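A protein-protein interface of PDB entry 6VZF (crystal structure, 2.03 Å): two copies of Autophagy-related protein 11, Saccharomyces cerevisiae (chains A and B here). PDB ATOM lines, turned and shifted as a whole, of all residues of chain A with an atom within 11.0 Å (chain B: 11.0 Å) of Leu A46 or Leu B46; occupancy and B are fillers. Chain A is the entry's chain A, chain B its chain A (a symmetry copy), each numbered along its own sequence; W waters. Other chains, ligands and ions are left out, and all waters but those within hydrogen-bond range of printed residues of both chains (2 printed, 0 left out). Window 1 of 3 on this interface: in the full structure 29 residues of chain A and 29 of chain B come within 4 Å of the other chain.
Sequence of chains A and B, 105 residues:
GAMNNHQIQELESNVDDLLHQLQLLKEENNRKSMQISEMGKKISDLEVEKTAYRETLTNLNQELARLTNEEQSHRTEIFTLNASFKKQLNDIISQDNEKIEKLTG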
ATOM      1  N   GLU A  38       1.850   5.646  26.601  1.00  0.00           N
ATOM      2  CA  GLU A  38       1.507   4.312  26.081  1.00  0.00           C
ATOM      3  C   GLU A  38       2.756   3.632  25.478  1.00  0.00           C
ATOM      4  O   GLU A  38       2.863   2.415  25.625  1.00  0.00           O
ATOM      5  CB  GLU A  38       0.425   4.461  25.031  1.00  0.00           C
ATOM      6  CG  GLU A  38      -0.877   4.968  25.629  1.00  0.00           C
ATOM      7  CD  GLU A  38      -1.952   5.307  24.606  1.00  0.00           C
ATOM      8  OE1 GLU A  38      -3.097   5.597  25.033  1.00  0.00           O
ATOM      9  OE2 GLU A  38      -1.644   5.307  23.383  1.00  0.00           O
ATOM     10  N   MET A  39       3.617   4.380  24.779  1.00  0.00           N
ATOM     11  CA  MET A  39       4.854   3.868  24.150  1.00  0.00           C
ATOM     12  C   MET A  39       5.872   3.606  25.239  1.00  0.00           C
ATOM     13  O   MET A  39       6.517   2.600  25.123  1.00  0.00           O
ATOM     14  CB  MET A  39       5.420   4.824  23.111  1.00  0.00           C
ATOM     15  CG  MET A  39       4.588   4.805  21.860  1.00  0.00           C
ATOM     16  SD  MET A  39       5.152   6.157  20.695  1.00  0.00           S
ATOM     17  CE  MET A  39       6.014   5.182  19.473  1.00  0.00           C
ATOM     18  N   GLY A  40       5.987   4.457  26.260  1.00  0.00           N
ATOM     19  CA  GLY A  40       6.848   4.212  27.418  1.00  0.00           C
ATOM     20  C   GLY A  40       6.533   2.848  28.078  1.00  0.00           C
ATOM     21  O   GLY A  40       7.487   2.074  28.465  1.00  0.00           O
ATOM     22  N   LYS A  41       5.264   2.603  28.339  1.00  0.00           N
ATOM     23  CA  LYS A  41       4.753   1.326  28.878  1.00  0.00           C
ATOM     24  C   LYS A  41       4.999   0.126  27.941  1.00  0.00           C
ATOM     25  O   LYS A  41       5.405  -0.883  28.436  1.00  0.00           O
ATOM     26  CB  LYS A  41       3.269   1.451  29.201  1.00  0.00           C
ATOM     27  CG  LYS A  41       3.080   2.209  30.503  1.00  0.00           C
ATOM     28  CD  LYS A  41       1.687   2.786  30.727  1.00  0.00           C
ATOM     29  CE  LYS A  41       1.729   3.993  31.639  1.00  0.00           C
ATOM     30  NZ  LYS A  41       0.484   4.789  31.544  1.00  0.00           N
ATOM     31  N   LYS A  42       4.660   0.210  26.683  1.00  0.00           N
ATOM     32  CA  LYS A  42       5.000  -0.813  25.697  1.00  0.00           C
ATOM     33  C   LYS A  42       6.507  -1.120  25.745  1.00  0.00           C
ATOM     34  O   LYS A  42       6.869  -2.330  25.720  1.00  0.00           O
ATOM     35  CB  LYS A  42       4.462  -0.397  24.352  1.00  0.00           C
ATOM     36  CG  LYS A  42       4.641  -1.361  23.233  1.00  0.00           C
ATOM     37  CD  LYS A  42       4.104  -2.759  23.578  1.00  0.00           C
ATOM     38  CE  LYS A  42       3.610  -3.512  22.365  1.00  0.00           C
ATOM     39  NZ  LYS A  42       3.126  -4.869  22.747  1.00  0.00           N
ATOM     40  N   ILE A  43       7.374  -0.141  25.896  1.00  0.00           N
ATOM     41  CA  ILE A  43       8.827  -0.371  25.891  1.00  0.00           C
ATOM     42  C   ILE A  43       9.198  -1.155  27.144  1.00  0.00           C
ATOM     43  O   ILE A  43      10.054  -2.062  27.063  1.00  0.00           O
ATOM     44  CB  ILE A  43       9.626   0.935  25.756  1.00  0.00           C
ATOM     45  CG1 ILE A  43       9.576   1.416  24.319  1.00  0.00           C
ATOM     46  CG2 ILE A  43      11.036   0.810  26.265  1.00  0.00           C
ATOM     47  CD1 ILE A  43      10.095   2.833  24.147  1.00  0.00           C
ATOM     48  N   SER A  44       8.695  -0.769  28.289  1.00  0.00           N
ATOM     49  CA  SER A  44       8.954  -1.491  29.543  1.00  0.00           C
ATOM     50  C   SER A  44       8.468  -2.947  29.453  1.00  0.00           C
ATOM     51  O   SER A  44       9.174  -3.794  29.993  1.00  0.00           O
ATOM     52  CB  SER A  44       8.266  -0.794  30.756  1.00  0.00           C
ATOM     53  OG  SER A  44       8.900   0.463  30.910  1.00  0.00           O
ATOM     54  N   ASP A  45       7.250  -3.140  28.966  1.00  0.00           N
ATOM     55  CA  ASP A  45       6.657  -4.480  28.763  1.00  0.00           C
ATOM     56  C   ASP A  45       7.556  -5.322  27.830  1.00  0.00           C
ATOM     57  O   ASP A  45       7.932  -6.376  28.211  1.00  0.00           O
ATOM     58  CB  ASP A  45       5.255  -4.385  28.222  1.00  0.00           C
ATOM     59  CG  ASP A  45       4.284  -3.680  29.214  1.00  0.00           C
ATOM     60  OD1 ASP A  45       4.685  -3.305  30.387  1.00  0.00           O
ATOM     61  OD2 ASP A  45       3.160  -3.468  28.787  1.00  0.00           O
ATOM     62  N   LEU A  46       7.943  -4.816  26.688  1.00  0.00           N
ATOM     63  CA  LEU A  46       8.768  -5.564  25.717  1.00  0.00           C
ATOM     64  C   LEU A  46      10.136  -5.869  26.333  1.00  0.00           C
ATOM     65  O   LEU A  46      10.634  -6.968  26.112  1.00  0.00           O
ATOM     66  CB  LEU A  46       8.912  -4.818  24.405  1.00  0.00           C
ATOM     67  CG  LEU A  46       7.729  -4.832  23.514  1.00  0.00           C
ATOM     68  CD1 LEU A  46       7.929  -3.798  22.387  1.00  0.00           C
ATOM     69  CD2 LEU A  46       7.385  -6.195  22.973  1.00  0.00           C
ATOM     70  N   GLU A  47      10.709  -4.964  27.073  1.00  0.00           N
ATOM     71  CA  GLU A  47      12.017  -5.153  27.717  1.00  0.00           C
ATOM     72  C   GLU A  47      11.975  -6.325  28.686  1.00  0.00           C
ATOM     73  O   GLU A  47      12.939  -7.116  28.659  1.00  0.00           O
ATOM     74  CB  GLU A  47      12.480  -3.910  28.472  1.00  0.00           C
ATOM     75  CG  GLU A  47      12.995  -2.860  27.531  1.00  0.00           C
ATOM     76  CD  GLU A  47      13.489  -1.569  28.176  1.00  0.00           C
ATOM     77  OE1 GLU A  47      12.970  -1.213  29.276  1.00  0.00           O
ATOM     78  OE2 GLU A  47      14.398  -0.923  27.545  1.00  0.00           O
ATOM     79  N   VAL A  48      10.956  -6.384  29.567  1.00  0.00           N
ATOM     80  CA  VAL A  48      10.908  -7.494  30.540  1.00  0.00           C
ATOM     81  C   VAL A  48      10.513  -8.793  29.789  1.00  0.00           C
ATOM     82  O   VAL A  48      10.972  -9.832  30.193  1.00  0.00           O
ATOM     83  CB  VAL A  48      10.066  -7.127  31.789  1.00  0.00           C
ATOM     84  CG1 VAL A  48       8.590  -7.111  31.504  1.00  0.00           C
ATOM     85  CG2 VAL A  48      10.390  -8.097  32.933  1.00  0.00           C
ATOM     86  N   GLU A  49       9.697  -8.765  28.747  1.00  0.00           N
ATOM     87  CA  GLU A  49       9.331  -9.992  28.006  1.00  0.00           C
ATOM     88  C   GLU A  49      10.580 -10.530  27.281  1.00  0.00           C
ATOM     89  O   GLU A  49      10.825 -11.715  27.342  1.00  0.00           O
ATOM     90  CB  GLU A  49       8.186  -9.755  27.063  1.00  0.00           C
ATOM     91  CG  GLU A  49       6.914  -9.454  27.767  1.00  0.00           C
ATOM     92  CD  GLU A  49       5.855  -8.728  26.867  1.00  0.00           C
ATOM     93  OE1 GLU A  49       6.089  -8.461  25.683  1.00  0.00           O
ATOM     94  OE2 GLU A  49       4.777  -8.447  27.360  1.00  0.00           O
ATOM     95  N   LYS A  50      11.363  -9.654  26.664  1.00  0.00           N
ATOM     96  CA  LYS A  50      12.648 -10.001  26.061  1.00  0.00           C
ATOM     97  C   LYS A  50      13.591 -10.632  27.100  1.00  0.00           C
ATOM     98  O   LYS A  50      14.139 -11.713  26.831  1.00  0.00           O
ATOM     99  CB  LYS A  50      13.229  -8.811  25.357  1.00  0.00           C
ATOM    100  CG  LYS A  50      14.598  -9.044  24.726  1.00  0.00           C
ATOM    101  CD  LYS A  50      15.314  -7.761  24.395  1.00  0.00           C
ATOM    102  CE  LYS A  50      16.775  -7.968  24.072  1.00  0.00           C
ATOM    103  NZ  LYS A  50      17.369  -6.634  23.804  1.00  0.00           N
ATOM    104  N   THR A  51      13.686 -10.090  28.272  1.00  0.00           N
ATOM    105  CA  THR A  51      14.522 -10.619  29.372  1.00  0.00           C
ATOM    106  C   THR A  51      14.003 -11.996  29.734  1.00  0.00           C
ATOM    107  O   THR A  51      14.826 -12.879  29.935  1.00  0.00           O
ATOM    108  CB  THR A  51      14.476  -9.676  30.582  1.00  0.00           C
ATOM    109  OG1 THR A  51      15.107  -8.486  30.118  1.00  0.00           O
ATOM    110  CG2 THR A  51      15.144 -10.225  31.812  1.00  0.00           C
ATOM    111  N   ALA A  52      12.694 -12.191  29.831  1.00  0.00           N
ATOM    112  CA  ALA A  52      12.165 -13.511  30.248  1.00  0.00           C
ATOM    113  C   ALA A  52      12.615 -14.553  29.224  1.00  0.00           C
ATOM    114  O   ALA A  52      13.035 -15.603  29.656  1.00  0.00           O
ATOM    115  CB  ALA A  52      10.668 -13.476  30.414  1.00  0.00           C
ATOM    116  N   TYR A  53      12.479 -14.293  27.926  1.00  0.00           N
ATOM    117  CA  TYR A  53      12.871 -15.239  26.878  1.00  0.00           C
ATOM    118  C   TYR A  53      14.379 -15.457  26.874  1.00  0.00           C
ATOM    119  O   TYR A  53      14.840 -16.625  26.788  1.00  0.00           O
ATOM    120  CB  TYR A  53      12.344 -14.862  25.521  1.00  0.00           C
ATOM    121  CG  TYR A  53      10.846 -14.999  25.409  1.00  0.00           C
ATOM    122  CD1 TYR A  53      10.134 -15.898  26.171  1.00  0.00           C
ATOM    123  CD2 TYR A  53      10.132 -14.261  24.530  1.00  0.00           C
ATOM    124  CE1 TYR A  53       8.772 -16.084  26.022  1.00  0.00           C
ATOM    125  CE2 TYR A  53       8.753 -14.368  24.423  1.00  0.00           C
ATOM    126  CZ  TYR A  53       8.062 -15.310  25.146  1.00  0.00           C
ATOM    127  OH  TYR A  53       6.733 -15.526  24.923  1.00  0.00           O
ATOM    128  N   ARG A  54      15.151 -14.412  27.107  1.00  0.00           N
ATOM    129  CA  ARG A  54      16.615 -14.509  27.052  1.00  0.00           C
ATOM    130  C   ARG A  54      17.125 -15.412  28.195  1.00  0.00           C
ATOM    131  O   ARG A  54      17.995 -16.184  27.996  1.00  0.00           O
ATOM    132  CB  ARG A  54      17.237 -13.121  27.210  1.00  0.00           C
ATOM    133  CG  ARG A  54      18.750 -13.166  27.031  1.00  0.00           C
ATOM    134  CD  ARG A  54      19.551 -11.884  27.178  1.00  0.00           C
ATOM    135  NE  ARG A  54      19.185 -11.270  28.374  1.00  0.00           N
ATOM    136  CZ  ARG A  54      18.599 -10.061  28.510  1.00  0.00           C
ATOM    137  NH1 ARG A  54      18.413  -9.194  27.512  1.00  0.00           N
ATOM    138  NH2 ARG A  54      18.260  -9.693  29.728  1.00  0.00           N
ATOM    139  N   GLU A  55      16.606 -15.236  29.396  1.00  0.00           N
ATOM    140  CA  GLU A  55      17.056 -15.925  30.622  1.00  0.00           C
ATOM    141  C   GLU A  55      16.657 -17.384  30.571  1.00  0.00           C
ATOM    142  O   GLU A  55      17.494 -18.262  30.893  1.00  0.00           O
ATOM    143  CB  GLU A  55      16.447 -15.218  31.820  1.00  0.00           C
ATOM    144  CG  GLU A  55      17.092 -13.884  32.010  1.00  0.00           C
ATOM    145  CD  GLU A  55      16.608 -13.166  33.256  1.00  0.00           C
ATOM    146  OE1 GLU A  55      15.512 -13.555  33.789  1.00  0.00           O
ATOM    147  OE2 GLU A  55      17.328 -12.226  33.702  1.00  0.00           O
ATOM    148  N   GLU B  38      11.850   8.079  17.980  1.00  0.00           N
ATOM    149  CA  GLU B  38      12.872   7.293  18.690  1.00  0.00           C
ATOM    150  C   GLU B  38      12.216   6.125  19.459  1.00  0.00           C
ATOM    151  O   GLU B  38      12.838   5.065  19.516  1.00  0.00           O
ATOM    152  CB  GLU B  38      13.613   8.206  19.645  1.00  0.00           C
ATOM    153  CG  GLU B  38      14.413   9.267  18.907  1.00  0.00           C
ATOM    154  CD  GLU B  38      15.040  10.324  19.804  1.00  0.00           C
ATOM    155  OE1 GLU B  38      15.827  11.148  19.277  1.00  0.00           O
ATOM    156  OE2 GLU B  38      14.726  10.344  21.025  1.00  0.00           O
ATOM    157  N   MET B  39      11.045   6.340  20.071  1.00  0.00           N
ATOM    158  CA  MET B  39      10.301   5.317  20.838  1.00  0.00           C
ATOM    159  C   MET B  39       9.679   4.344  19.860  1.00  0.00           C
ATOM    160  O   MET B  39       9.728   3.185  20.170  1.00  0.00           O
ATOM    161  CB  MET B  39       9.234   5.923  21.737  1.00  0.00           C
ATOM    162  CG  MET B  39       9.858   6.591  22.930  1.00  0.00           C
ATOM    163  SD  MET B  39       8.558   7.535  23.889  1.00  0.00           S
ATOM    164  CE  MET B  39       8.354   6.455  25.295  1.00  0.00           C
ATOM    165  N   GLY B  40       9.147   4.794  18.722  1.00  0.00           N
ATOM    166  CA  GLY B  40       8.646   3.914  17.665  1.00  0.00           C
ATOM    167  C   GLY B  40       9.724   2.897  17.218  1.00  0.00           C
ATOM    168  O   GLY B  40       9.413   1.665  17.011  1.00  0.00           O
ATOM    169  N   LYS B  41      10.913   3.392  16.935  1.00  0.00           N
ATOM    170  CA  LYS B  41      12.095   2.578  16.583  1.00  0.00           C
ATOM    171  C   LYS B  41      12.539   1.626  17.714  1.00  0.00           C
ATOM    172  O   LYS B  41      12.815   0.504  17.409  1.00  0.00           O
ATOM    173  CB  LYS B  41      13.249   3.482  16.168  1.00  0.00           C
ATOM    174  CG  LYS B  41      13.032   3.988  14.753  1.00  0.00           C
ATOM    175  CD  LYS B  41      13.847   5.218  14.367  1.00  0.00           C
ATOM    176  CE  LYS B  41      13.163   6.012  13.275  1.00  0.00           C
ATOM    177  NZ  LYS B  41      13.713   7.383  13.176  1.00  0.00           N
ATOM    178  N   LYS B  42      12.701   2.092  18.922  1.00  0.00           N
ATOM    179  CA  LYS B  42      12.964   1.237  20.076  1.00  0.00           C
ATOM    180  C   LYS B  42      11.915   0.113  20.157  1.00  0.00           C
ATOM    181  O   LYS B  42      12.317  -1.060  20.396  1.00  0.00           O
ATOM    182  CB  LYS B  42      13.093   2.097  21.307  1.00  0.00           C
ATOM    183  CG  LYS B  42      13.445   1.402  22.575  1.00  0.00           C
ATOM    184  CD  LYS B  42      14.708   0.538  22.433  1.00  0.00           C
ATOM    185  CE  LYS B  42      15.482   0.416  23.724  1.00  0.00           C
ATOM    186  NZ  LYS B  42      16.680  -0.453  23.541  1.00  0.00           N
ATOM    187  N   ILE B  43      10.651   0.372  19.895  1.00  0.00           N
ATOM    188  CA  ILE B  43       9.600  -0.651  20.012  1.00  0.00           C
ATOM    189  C   ILE B  43       9.815  -1.694  18.923  1.00  0.00           C
ATOM    190  O   ILE B  43       9.636  -2.901  19.193  1.00  0.00           O
ATOM    191  CB  ILE B  43       8.187  -0.044  19.975  1.00  0.00           C
ATOM    192  CG1 ILE B  43       7.876   0.602  21.311  1.00  0.00           C
ATOM    193  CG2 ILE B  43       7.137  -1.041  19.567  1.00  0.00           C
ATOM    194  CD1 ILE B  43       6.627   1.464  21.279  1.00  0.00           C
ATOM    195  N   SER B  44      10.062  -1.280  17.706  1.00  0.00           N
ATOM    196  CA  SER B  44      10.332  -2.210  16.600  1.00  0.00           C
ATOM    197  C   SER B  44      11.564  -3.079  16.899  1.00  0.00           C
ATOM    198  O   SER B  44      11.505  -4.253  16.540  1.00  0.00           O
ATOM    199  CB  SER B  44      10.553  -1.450  15.256  1.00  0.00           C
ATOM    200  OG  SER B  44       9.319  -0.836  14.935  1.00  0.00           O
ATOM    201  N   ASP B  45      12.643  -2.453  17.347  1.00  0.00           N
ATOM    202  CA  ASP B  45      13.889  -3.151  17.732  1.00  0.00           C
ATOM    203  C   ASP B  45      13.594  -4.192  18.835  1.00  0.00           C
ATOM    204  O   ASP B  45      13.915  -5.315  18.649  1.00  0.00           O
ATOM    205  CB  ASP B  45      14.949  -2.178  18.178  1.00  0.00           C
ATOM    206  CG  ASP B  45      15.384  -1.213  17.036  1.00  0.00           C
ATOM    207  OD1 ASP B  45      14.902  -1.334  15.841  1.00  0.00           O
ATOM    208  OD2 ASP B  45      16.155  -0.326  17.365  1.00  0.00           O
ATOM    209  N   LEU B  46      12.928  -3.827  19.898  1.00  0.00           N
ATOM    210  CA  LEU B  46      12.636  -4.745  21.018  1.00  0.00           C
ATOM    211  C   LEU B  46      11.730  -5.878  20.532  1.00  0.00           C
ATOM    212  O   LEU B  46      11.946  -7.009  20.953  1.00  0.00           O
ATOM    213  CB  LEU B  46      12.021  -4.019  22.199  1.00  0.00           C
ATOM    214  CG  LEU B  46      12.946  -3.204  23.018  1.00  0.00           C
ATOM    215  CD1 LEU B  46      12.129  -2.309  23.972  1.00  0.00           C
ATOM    216  CD2 LEU B  46      13.986  -4.009  23.754  1.00  0.00           C
ATOM    217  N   GLU B  47      10.779  -5.604  19.686  1.00  0.00           N
ATOM    218  CA  GLU B  47       9.855  -6.614  19.149  1.00  0.00           C
ATOM    219  C   GLU B  47      10.616  -7.684  18.381  1.00  0.00           C
ATOM    220  O   GLU B  47      10.285  -8.870  18.585  1.00  0.00           O
ATOM    221  CB  GLU B  47       8.799  -6.008  18.229  1.00  0.00           C
ATOM    222  CG  GLU B  47       7.725  -5.314  19.014  1.00  0.00           C
ATOM    223  CD  GLU B  47       6.610  -4.669  18.195  1.00  0.00           C
ATOM    224  OE1 GLU B  47       6.885  -4.262  17.027  1.00  0.00           O
ATOM    225  OE2 GLU B  47       5.464  -4.575  18.759  1.00  0.00           O
ATOM    226  N   VAL B  48      11.526  -7.286  17.470  1.00  0.00           N
ATOM    227  CA  VAL B  48      12.256  -8.304  16.688  1.00  0.00           C
ATOM    228  C   VAL B  48      13.289  -8.994  17.617  1.00  0.00           C
ATOM    229  O   VAL B  48      13.536 -10.156  17.410  1.00  0.00           O
ATOM    230  CB  VAL B  48      12.795  -7.725  15.354  1.00  0.00           C
ATOM    231  CG1 VAL B  48      13.974  -6.815  15.556  1.00  0.00           C
ATOM    232  CG2 VAL B  48      13.150  -8.874  14.400  1.00  0.00           C
ATOM    233  N   GLU B  49      13.884  -8.333  18.598  1.00  0.00           N
ATOM    234  CA  GLU B  49      14.852  -8.984  19.507  1.00  0.00           C
ATOM    235  C   GLU B  49      14.107 -10.018  20.373  1.00  0.00           C
ATOM    236  O   GLU B  49      14.594 -11.118  20.517  1.00  0.00           O
ATOM    237  CB  GLU B  49      15.599  -7.981  20.338  1.00  0.00           C
ATOM    238  CG  GLU B  49      16.499  -7.119  19.531  1.00  0.00           C
ATOM    239  CD  GLU B  49      16.896  -5.782  20.245  1.00  0.00           C
ATOM    240  OE1 GLU B  49      16.490  -5.512  21.381  1.00  0.00           O
ATOM    241  OE2 GLU B  49      17.638  -5.014  19.658  1.00  0.00           O
ATOM    242  N   LYS B  50      12.932  -9.670  20.880  1.00  0.00           N
ATOM    243  CA  LYS B  50      12.053 -10.591  21.597  1.00  0.00           C
ATOM    244  C   LYS B  50      11.703 -11.809  20.723  1.00  0.00           C
ATOM    245  O   LYS B  50      11.866 -12.947  21.191  1.00  0.00           O
ATOM    246  CB  LYS B  50      10.857  -9.861  22.128  1.00  0.00           C
ATOM    247  CG  LYS B  50       9.843 -10.736  22.858  1.00  0.00           C
ATOM    248  CD  LYS B  50       8.501 -10.068  23.015  1.00  0.00           C
ATOM    249  CE  LYS B  50       7.414 -11.026  23.443  1.00  0.00           C
ATOM    250  NZ  LYS B  50       6.146 -10.258  23.522  1.00  0.00           N
ATOM    251  N   THR B  51      11.373 -11.619  19.486  1.00  0.00           N
ATOM    252  CA  THR B  51      11.055 -12.702  18.530  1.00  0.00           C
ATOM    253  C   THR B  51      12.291 -13.564  18.369  1.00  0.00           C
ATOM    254  O   THR B  51      12.141 -14.778  18.356  1.00  0.00           O
ATOM    255  CB  THR B  51      10.610 -12.117  17.183  1.00  0.00           C
ATOM    256  OG1 THR B  51       9.385 -11.453  17.482  1.00  0.00           O
ATOM    257  CG2 THR B  51      10.446 -13.140  16.094  1.00  0.00           C
ATOM    258  N   ALA B  52      13.475 -12.980  18.237  1.00  0.00           N
ATOM    259  CA  ALA B  52      14.690 -13.799  18.012  1.00  0.00           C
ATOM    260  C   ALA B  52      14.871 -14.727  19.212  1.00  0.00           C
ATOM    261  O   ALA B  52      15.158 -15.879  18.978  1.00  0.00           O
ATOM    262  CB  ALA B  52      15.898 -12.933  17.765  1.00  0.00           C
ATOM    263  N   TYR B  53      14.766 -14.231  20.443  1.00  0.00           N
ATOM    264  CA  TYR B  53      14.938 -15.046  21.648  1.00  0.00           C
ATOM    265  C   TYR B  53      13.835 -16.090  21.766  1.00  0.00           C
ATOM    266  O   TYR B  53      14.128 -17.277  22.063  1.00  0.00           O
ATOM    267  CB  TYR B  53      15.079 -14.220  22.898  1.00  0.00           C
ATOM    268  CG  TYR B  53      16.374 -13.447  22.953  1.00  0.00           C
ATOM    269  CD1 TYR B  53      17.512 -13.879  22.310  1.00  0.00           C
ATOM    270  CD2 TYR B  53      16.484 -12.302  23.664  1.00  0.00           C
ATOM    271  CE1 TYR B  53      18.721 -13.218  22.417  1.00  0.00           C
ATOM    272  CE2 TYR B  53      17.664 -11.575  23.714  1.00  0.00           C
ATOM    273  CZ  TYR B  53      18.808 -12.047  23.118  1.00  0.00           C
ATOM    274  OH  TYR B  53      20.004 -11.416  23.304  1.00  0.00           O
ATOM    275  N   ARG B  54      12.614 -15.736  21.408  1.00  0.00           N
ATOM    276  CA  ARG B  54      11.474 -16.651  21.553  1.00  0.00           C
ATOM    277  C   ARG B  54      11.639 -17.852  20.599  1.00  0.00           C
ATOM    278  O   ARG B  54      11.365 -18.940  20.964  1.00  0.00           O
ATOM    279  CB  ARG B  54      10.174 -15.924  21.205  1.00  0.00           C
ATOM    280  CG  ARG B  54       8.957 -16.804  21.468  1.00  0.00           C
ATOM    281  CD  ARG B  54       7.572 -16.264  21.157  1.00  0.00           C
ATOM    282  NE  ARG B  54       7.579 -15.755  19.861  1.00  0.00           N
ATOM    283  CZ  ARG B  54       7.365 -14.470  19.501  1.00  0.00           C
ATOM    284  NH1 ARG B  54       6.964 -13.508  20.335  1.00  0.00           N
ATOM    285  NH2 ARG B  54       7.492 -14.176  18.224  1.00  0.00           N
ATOM    286  N   GLU B  55      12.022 -17.605  19.360  1.00  0.00           N
ATOM    287  CA  GLU B  55      12.117 -18.615  18.286  1.00  0.00           C
ATOM    288  C   GLU B  55      13.281 -19.544  18.551  1.00  0.00           C
ATOM    289  O   GLU B  55      13.123 -20.782  18.419  1.00  0.00           O
ATOM    290  CB  GLU B  55      12.267 -17.890  16.960  1.00  0.00           C
ATOM    291  CG  GLU B  55      10.981 -17.226  16.591  1.00  0.00           C
ATOM    292  CD  GLU B  55      11.025 -16.573  15.222  1.00  0.00           C
ATOM    293  OE1 GLU B  55      12.171 -16.337  14.702  1.00  0.00           O
ATOM    294  OE2 GLU B  55       9.919 -16.308  14.667  1.00  0.00           O
HETATM  295  O   HOH W   1      16.249  -1.802  26.295  1.00  0.00           O
HETATM  296  O   HOH W   2       4.398  -6.146  20.229  1.00  0.00           O
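The side-chain hydroxyl of Ser A44 lies within hydrogen-bond range of the backbone carbonyl oxygen of Gly A40, at 3.3 Å. The side-chain hydroxyl (OG1) of Thr A51 lies within hydrogen-bond range of the backbone carbonyl oxygen (O) of Glu A47 (3.0 Å). NH2 of Arg A54 lies within hydrogen-bond range of OG1 of Thr A51, at 3.4 Å. OG of Ser B44 sits at hydrogen-bond distance from O of Gly B40 (3.3 Å). The side-chain hydroxyl of Thr B51 sits at hydrogen-bond distance from the guanidinium group of Arg B54 (3.4 Å).
The side-chain carboxylate (OE1) of Glu A49 lies within salt-bridge range of the side-chain amino group (NZ) of Lys B50 (2.8 Å). OE1 of Glu B49 lies within salt-bridge range of NZ of Lys A50 (2.8 Å).
Hydrophobic or aromatic side chains of chain A that line the printed part of chain B: Met A39, Ile A43, Leu A46 and Tyr A53. Of the 18 printed residues of chain B, 10 touch a printed residue of chain A. Hydrophobic or aromatic side chains of chain B that line the printed part of chain A: Met B39, Ile B43, Leu B46 and Tyr B53. Among the printed residues, 20 pairs touch across the chains. Among the printed residues, Asp or Glu carboxylates within 4 Å of a Lys or Arg side-chain nitrogen of the other chain: Glu A49 with Lys B50 (2.8 Å) and Lys A50 with Glu B49 (2.8 Å).
Water W1 bridges the side-chain carboxylate (OE2) of Glu A47 and the side-chain amino group (NZ) of Lys B42. Water W2 bridges OE2 of Glu B47 (2.4 Å) and NZ of Lys A42 (3.1 Å).
Met A39 touches Gly B40, and with the chains exchanged Gly A40 touches Met B39. Glu A49 touches Lys B50, and with the chains exchanged Lys A50 touches Glu B49. Lys A50 touches Tyr B53, and with the chains exchanged Tyr A53 touches Lys B50. Tyr A53 touches Arg B54, and with the chains exchanged Arg A54 touches Tyr B53. 18 positions are printed for both chains. Of the 20 pairs that touch across the chains among the printed residues, 20 have their exchanged pair printed and touching as well.
Among the printed residues, pairs that only touch across the chains: Met A39 with Met B39 (3.8 Å), Met A39 with Gly B40 (3.2 Å), Met A39 with Ile B43 (3.96 Å), Gly A40 with Met B39 (3.2 Å), Lys A42 with Ile B43 (3.97 Å), Ile A43 with Met B39 (3.96 Å), Ile A43 with Lys B42 (3.97 Å), Ile A43 with Ile B43 (3.5 Å), Ile A43 with Leu B46 (3.7 Å), Leu A46 with Ile B43 (3.7 Å), Leu A46 with Leu B46 (3.9 Å), Leu A46 with Glu B47 (3.7 Å), Glu A47 with Leu B46 (3.7 Å), Lys A50 with Tyr B53 (3.7 Å), Tyr A53 with Lys B50 (3.7 Å), Tyr A53 with Tyr B53 (3.8 Å), Tyr A53 with Arg B54 (3.7 Å) and Arg A54 with Tyr B53 (3.7 Å).
Of chain A, only Ile A43 (3.7 Å), Leu A46 (3.9 Å) and Glu A47 (3.7 Å) come within 4 Å of Leu B46. Of chain B, only Ile B43 comes within 4 Å of Lys A42. Ser A44 touches none of the printed residues of chain B. Val A48 touches none of the printed residues of chain B. Glu A49 touches just one residue of chain B: Lys B50. Of chain B, only Glu B49 (2.8 Å) and Tyr B53 (3.7 Å) come within 4 Å of Lys A50. Of the printed residues of chain A, Lys B42 touches Ile A43. Of the printed residues of chain A, Ile B43 touches Met A39 (3.96 Å), Lys A42 (3.97 Å), Ile A43 (3.5 Å) and Leu A46 (3.7 Å). No residue of chain A comes within 4 Å of Asp B45. Glu B47 touches one residue of chain A. Of the printed residues of chain B, Tyr A53 touches Lys B50, Tyr B53 and Arg B54. Thr B51 touches none of the printed residues of chain A. The nearest residue of chain B that does not touch Leu A46 is Lys B50 (4.03 Å). The nearest residue of chain A that does not touch Leu B46 is Lys A50 (4.03 Å). The nearest printed residue of chain B that does not touch Gly A40 is Ile B43 (5.8 Å).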
